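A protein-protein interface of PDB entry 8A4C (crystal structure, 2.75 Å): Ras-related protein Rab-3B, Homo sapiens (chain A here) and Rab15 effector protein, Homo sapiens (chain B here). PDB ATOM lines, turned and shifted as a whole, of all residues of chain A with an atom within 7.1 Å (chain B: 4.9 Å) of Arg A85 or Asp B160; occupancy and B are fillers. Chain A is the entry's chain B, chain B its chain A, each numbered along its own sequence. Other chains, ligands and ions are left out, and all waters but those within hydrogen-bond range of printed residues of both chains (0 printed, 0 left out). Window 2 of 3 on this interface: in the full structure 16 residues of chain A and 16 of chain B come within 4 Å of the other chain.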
ATOM      1  N   GLY A  82      20.149 -36.210  -2.367  1.00  0.00           N
ATOM      2  CA  GLY A  82      18.907 -35.956  -3.078  1.00  0.00           C
ATOM      3  C   GLY A  82      18.139 -34.729  -2.628  1.00  0.00           C
ATOM      4  O   GLY A  82      17.278 -34.251  -3.375  1.00  0.00           O
ATOM      5  N   GLN A  83      18.430 -34.211  -1.434  1.00  0.00           N
ATOM      6  CA  GLN A  83      17.723 -33.048  -0.908  1.00  0.00           C
ATOM      7  C   GLN A  83      18.037 -31.808  -1.737  1.00  0.00           C
ATOM      8  O   GLN A  83      19.126 -31.673  -2.306  1.00  0.00           O
ATOM      9  CB  GLN A  83      18.099 -32.802   0.556  1.00  0.00           C
ATOM     10  CG  GLN A  83      17.686 -33.914   1.519  1.00  0.00           C
ATOM     11  CD  GLN A  83      18.163 -33.667   2.945  1.00  0.00           C
ATOM     12  OE1 GLN A  83      18.264 -32.524   3.395  1.00  0.00           O
ATOM     13  NE2 GLN A  83      18.481 -34.745   3.654  1.00  0.00           N
ATOM     14  N   GLU A  84      17.054 -30.900  -1.797  1.00  0.00           N
ATOM     15  CA  GLU A  84      17.109 -29.742  -2.686  1.00  0.00           C
ATOM     16  C   GLU A  84      18.225 -28.773  -2.312  1.00  0.00           C
ATOM     17  O   GLU A  84      18.842 -28.175  -3.203  1.00  0.00           O
ATOM     18  CB  GLU A  84      15.763 -29.025  -2.668  1.00  0.00           C
ATOM     19  CG  GLU A  84      15.449 -28.220  -3.917  1.00  0.00           C
ATOM     20  CD  GLU A  84      14.021 -27.694  -3.919  1.00  0.00           C
ATOM     21  OE1 GLU A  84      13.103 -28.448  -3.519  1.00  0.00           O
ATOM     22  OE2 GLU A  84      13.816 -26.527  -4.323  1.00  0.00           O
ATOM     23  N   ARG A  85      18.525 -28.637  -1.015  1.00  0.00           N
ATOM     24  CA  ARG A  85      19.515 -27.664  -0.563  1.00  0.00           C
ATOM     25  C   ARG A  85      20.936 -28.015  -0.985  1.00  0.00           C
ATOM     26  O   ARG A  85      21.805 -27.138  -0.952  1.00  0.00           O
ATOM     27  CB  ARG A  85      19.457 -27.514   0.959  1.00  0.00           C
ATOM     28  CG  ARG A  85      20.198 -28.587   1.723  1.00  0.00           C
ATOM     29  CD  ARG A  85      20.175 -28.360   3.220  1.00  0.00           C
ATOM     30  NE  ARG A  85      20.906 -27.168   3.634  1.00  0.00           N
ATOM     31  CZ  ARG A  85      20.341 -26.035   4.029  1.00  0.00           C
ATOM     32  NH1 ARG A  85      19.025 -25.895   4.073  1.00  0.00           N
ATOM     33  NH2 ARG A  85      21.118 -25.022   4.399  1.00  0.00           N
ATOM     34  N   TYR A  86      21.199 -29.266  -1.369  1.00  0.00           N
ATOM     35  CA  TYR A  86      22.501 -29.659  -1.888  1.00  0.00           C
ATOM     36  C   TYR A  86      22.515 -29.732  -3.409  1.00  0.00           C
ATOM     37  O   TYR A  86      23.543 -30.106  -3.992  1.00  0.00           O
ATOM     38  CB  TYR A  86      22.934 -30.994  -1.278  1.00  0.00           C
ATOM     39  CG  TYR A  86      22.856 -31.003   0.233  1.00  0.00           C
ATOM     40  CD1 TYR A  86      23.664 -30.160   0.992  1.00  0.00           C
ATOM     41  CD2 TYR A  86      21.967 -31.845   0.902  1.00  0.00           C
ATOM     42  CE1 TYR A  86      23.591 -30.152   2.376  1.00  0.00           C
ATOM     43  CE2 TYR A  86      21.888 -31.848   2.284  1.00  0.00           C
ATOM     44  CZ  TYR A  86      22.705 -30.999   3.017  1.00  0.00           C
ATOM     45  OH  TYR A  86      22.634 -30.994   4.393  1.00  0.00           O
ATOM     46  N   ARG A  87      21.409 -29.327  -4.055  1.00  0.00           N
ATOM     47  CA  ARG A  87      21.292 -29.386  -5.511  1.00  0.00           C
ATOM     48  C   ARG A  87      22.364 -28.561  -6.207  1.00  0.00           C
ATOM     49  O   ARG A  87      22.859 -28.962  -7.268  1.00  0.00           O
ATOM     50  CB  ARG A  87      19.906 -28.908  -5.944  1.00  0.00           C
ATOM     51  CG  ARG A  87      19.575 -29.218  -7.390  1.00  0.00           C
ATOM     52  CD  ARG A  87      19.534 -30.726  -7.623  1.00  0.00           C
ATOM     53  NE  ARG A  87      18.728 -31.409  -6.617  1.00  0.00           N
ATOM     54  CZ  ARG A  87      17.407 -31.525  -6.668  1.00  0.00           C
ATOM     55  NH1 ARG A  87      16.707 -31.019  -7.673  1.00  0.00           N
ATOM     56  NH2 ARG A  87      16.776 -32.176  -5.693  1.00  0.00           N
ATOM     57  N   THR A  88      22.755 -27.435  -5.608  1.00  0.00           N
ATOM     58  CA  THR A  88      23.861 -26.653  -6.144  1.00  0.00           C
ATOM     59  C   THR A  88      25.173 -27.427  -6.066  1.00  0.00           C
ATOM     60  O   THR A  88      25.829 -27.641  -7.097  1.00  0.00           O
ATOM     61  CB  THR A  88      23.966 -25.317  -5.405  1.00  0.00           C
ATOM     62  OG1 THR A  88      22.766 -24.568  -5.609  1.00  0.00           O
ATOM     63  CG2 THR A  88      25.122 -24.503  -5.933  1.00  0.00           C
ATOM     64  N   ILE A  89      25.523 -27.935  -4.872  1.00  0.00           N
ATOM     65  CA  ILE A  89      26.891 -28.421  -4.670  1.00  0.00           C
ATOM     66  C   ILE A  89      27.117 -29.719  -5.441  1.00  0.00           C
ATOM     67  O   ILE A  89      28.172 -29.900  -6.069  1.00  0.00           O
ATOM     68  CB  ILE A  89      27.237 -28.560  -3.167  1.00  0.00           C
ATOM     69  CG1 ILE A  89      28.614 -29.191  -2.979  1.00  0.00           C
ATOM     70  CG2 ILE A  89      26.238 -29.394  -2.401  1.00  0.00           C
ATOM     71  CD1 ILE A  89      29.291 -28.779  -1.721  1.00  0.00           C
ATOM     72  N   ILE B 106      15.452 -27.008   7.702  1.00  0.00           N
ATOM     73  CA  ILE B 106      16.787 -26.654   8.174  1.00  0.00           C
ATOM     74  C   ILE B 106      16.907 -25.137   8.250  1.00  0.00           C
ATOM     75  O   ILE B 106      16.718 -24.435   7.251  1.00  0.00           O
ATOM     76  CB  ILE B 106      17.862 -27.255   7.261  1.00  0.00           C
ATOM     77  CG1 ILE B 106      17.893 -28.770   7.451  1.00  0.00           C
ATOM     78  CG2 ILE B 106      19.231 -26.629   7.536  1.00  0.00           C
ATOM     79  CD1 ILE B 106      18.555 -29.502   6.332  1.00  0.00           C
ATOM     80  N   LYS B 107      17.235 -24.628   9.436  1.00  0.00           N
ATOM     81  CA  LYS B 107      17.399 -23.191   9.628  1.00  0.00           C
ATOM     82  C   LYS B 107      18.858 -22.761   9.635  1.00  0.00           C
ATOM     83  O   LYS B 107      19.156 -21.623   9.255  1.00  0.00           O
ATOM     84  CB  LYS B 107      16.747 -22.726  10.940  1.00  0.00           C
ATOM     85  CG  LYS B 107      15.386 -23.342  11.319  1.00  0.00           C
ATOM     86  CD  LYS B 107      14.326 -23.387  10.202  1.00  0.00           C
ATOM     87  CE  LYS B 107      13.306 -22.270  10.326  1.00  0.00           C
ATOM     88  NZ  LYS B 107      12.044 -22.638   9.625  1.00  0.00           N
ATOM     89  N   LEU B 108      19.775 -23.634  10.058  1.00  0.00           N
ATOM     90  CA  LEU B 108      21.181 -23.244  10.098  1.00  0.00           C
ATOM     91  C   LEU B 108      22.071 -24.453   9.841  1.00  0.00           C
ATOM     92  O   LEU B 108      21.703 -25.587  10.147  1.00  0.00           O
ATOM     93  CB  LEU B 108      21.528 -22.594  11.445  1.00  0.00           C
ATOM     94  CG  LEU B 108      22.873 -21.878  11.608  1.00  0.00           C
ATOM     95  CD1 LEU B 108      23.004 -20.727  10.618  1.00  0.00           C
ATOM     96  CD2 LEU B 108      23.051 -21.394  13.035  1.00  0.00           C
ATOM     97  N   GLN B 109      23.253 -24.202   9.278  1.00  0.00           N
ATOM     98  CA  GLN B 109      24.278 -25.234   9.148  1.00  0.00           C
ATOM     99  C   GLN B 109      25.637 -24.619   9.441  1.00  0.00           C
ATOM    100  O   GLN B 109      26.094 -23.742   8.705  1.00  0.00           O
ATOM    101  CB  GLN B 109      24.254 -25.871   7.755  1.00  0.00           C
ATOM    102  CG  GLN B 109      23.492 -27.189   7.733  1.00  0.00           C
ATOM    103  CD  GLN B 109      23.460 -27.848   6.371  1.00  0.00           C
ATOM    104  OE1 GLN B 109      23.487 -27.176   5.338  1.00  0.00           O
ATOM    105  NE2 GLN B 109      23.391 -29.175   6.362  1.00  0.00           N
ATOM    106  N   ILE B 157      26.624 -24.280  -0.546  1.00  0.00           N
ATOM    107  CA  ILE B 157      25.435 -24.684   0.208  1.00  0.00           C
ATOM    108  C   ILE B 157      24.415 -23.545   0.255  1.00  0.00           C
ATOM    109  O   ILE B 157      23.224 -23.747  -0.014  1.00  0.00           O
ATOM    110  CB  ILE B 157      25.809 -25.164   1.624  1.00  0.00           C
ATOM    111  CG1 ILE B 157      26.765 -26.363   1.579  1.00  0.00           C
ATOM    112  CG2 ILE B 157      24.557 -25.578   2.385  1.00  0.00           C
ATOM    113  CD1 ILE B 157      26.244 -27.562   0.832  1.00  0.00           C
ATOM    114  N   GLY B 158      24.861 -22.338   0.573  1.00  0.00           N
ATOM    115  CA  GLY B 158      23.978 -21.194   0.559  1.00  0.00           C
ATOM    116  C   GLY B 158      24.276 -20.247   1.701  1.00  0.00           C
ATOM    117  O   GLY B 158      25.270 -20.385   2.415  1.00  0.00           O
ATOM    118  N   GLU B 159      23.381 -19.268   1.871  1.00  0.00           N
ATOM    119  CA  GLU B 159      23.592 -18.194   2.836  1.00  0.00           C
ATOM    120  C   GLU B 159      23.374 -18.638   4.277  1.00  0.00           C
ATOM    121  O   GLU B 159      23.897 -17.994   5.192  1.00  0.00           O
ATOM    122  CB  GLU B 159      22.674 -17.016   2.514  1.00  0.00           C
ATOM    123  CG  GLU B 159      21.213 -17.403   2.340  1.00  0.00           C
ATOM    124  CD  GLU B 159      20.372 -16.273   1.779  1.00  0.00           C
ATOM    125  OE1 GLU B 159      20.833 -15.112   1.820  1.00  0.00           O
ATOM    126  OE2 GLU B 159      19.254 -16.545   1.294  1.00  0.00           O
ATOM    127  N   ASP B 160      22.617 -19.711   4.504  1.00  0.00           N
ATOM    128  CA  ASP B 160      22.366 -20.213   5.848  1.00  0.00           C
ATOM    129  C   ASP B 160      23.405 -21.233   6.302  1.00  0.00           C
ATOM    130  O   ASP B 160      23.197 -21.914   7.314  1.00  0.00           O
ATOM    131  CB  ASP B 160      20.959 -20.812   5.939  1.00  0.00           C
ATOM    132  CG  ASP B 160      20.714 -21.908   4.917  1.00  0.00           C
ATOM    133  OD1 ASP B 160      21.523 -22.062   3.974  1.00  0.00           O
ATOM    134  OD2 ASP B 160      19.688 -22.612   5.052  1.00  0.00           O
ATOM    135  N   CYS B 161      24.509 -21.360   5.574  1.00  0.00           N
ATOM    136  CA  CYS B 161      25.610 -22.232   5.955  1.00  0.00           C
ATOM    137  C   CYS B 161      26.808 -21.356   6.279  1.00  0.00           C
ATOM    138  O   CYS B 161      27.363 -20.698   5.392  1.00  0.00           O
ATOM    139  CB  CYS B 161      25.940 -23.219   4.843  1.00  0.00           C
ATOM    140  SG  CYS B 161      27.216 -24.418   5.282  1.00  0.00           S
ATOM    141  N   LEU B 162      27.204 -21.360   7.543  1.00  0.00           N
ATOM    142  CA  LEU B 162      28.319 -20.561   8.024  1.00  0.00           C
ATOM    143  C   LEU B 162      29.529 -21.454   8.255  1.00  0.00           C
ATOM    144  O   LEU B 162      29.397 -22.656   8.494  1.00  0.00           O
ATOM    145  CB  LEU B 162      27.953 -19.825   9.319  1.00  0.00           C
ATOM    146  CG  LEU B 162      27.200 -18.481   9.323  1.00  0.00           C
ATOM    147  CD1 LEU B 162      28.190 -17.331   9.177  1.00  0.00           C
ATOM    148  CD2 LEU B 162      26.065 -18.358   8.288  1.00  0.00           C
ATOM    149  N   LYS B 224      19.595 -14.609   9.975  1.00  0.00           N
ATOM    150  CA  LYS B 224      20.796 -15.295   9.509  1.00  0.00           C
ATOM    151  C   LYS B 224      22.029 -14.401   9.541  1.00  0.00           C
ATOM    152  O   LYS B 224      23.115 -14.861   9.912  1.00  0.00           O
ATOM    153  CB  LYS B 224      20.591 -15.817   8.083  1.00  0.00           C
ATOM    154  CG  LYS B 224      19.399 -16.736   7.900  1.00  0.00           C
ATOM    155  CD  LYS B 224      19.324 -17.240   6.466  1.00  0.00           C
ATOM    156  CE  LYS B 224      18.063 -18.056   6.230  1.00  0.00           C
ATOM    157  NZ  LYS B 224      17.983 -19.233   7.141  1.00  0.00           N
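The side-chain carboxylate (OD2) of Asp B160 lies within salt-bridge range of the guanidinium group (NH2) of Arg A85. OE1 of Gln B109 is in hydrogen-bond range of NE of Arg A85 (3.1 Å). The side-chain amide nitrogen (NE2) of Gln B109 lies within hydrogen-bond range of the side-chain hydroxyl (OH) of Tyr A86 (2.8 Å).
Arg A85 touches just these residues of chain B: Ile B106 (3.5 Å), Gln B109 (3.1 Å), Ile B157 (3.8 Å) and Asp B160 (2.9 Å). Of the printed residues of chain A, Ile B106 touches Arg A85. Leu B108 touches none of the printed residues of chain A. Printed residues of chain A within 4 Å of Ile B157: Arg A85, Tyr A86 and Ile A89. Asp B160 touches one residue of chain A. The nearest printed residue of chain A that does not touch Asp B160 is Tyr A86 (8.5 Å).
The side-chain sulfur (SG) of Cys B161 sits close to the backbone carbonyl oxygen (O) of Gln B109, at 3.7 Å. N of Leu B162 sits at hydrogen-bond distance from O of Gln B109 (2.9 Å). N of Gln B109 sits at hydrogen-bond distance from O of Asp B160.
Printed residues of chain A that touch a printed residue of chain B: Arg A85, Tyr A86 and Ile A89. Of the 11 printed residues of chain B, 4 touch a printed residue of chain A. Printed residues of chain B that touch a printed residue of chain A: Ile B106, Gln B109, Ile B157 and Asp B160. Hydrophobic or aromatic side chains of chain B that line the printed part of chain A: Ile B106 and Ile B157.
Among the printed residues, pairs that only touch across the chains: Arg A85 with Ile B106 (3.5 Å), Arg A85 with Ile B157 (3.8 Å), Tyr A86 with Ile B157 (3.7 Å) and Ile A89 with Ile B157 (3.7 Å).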
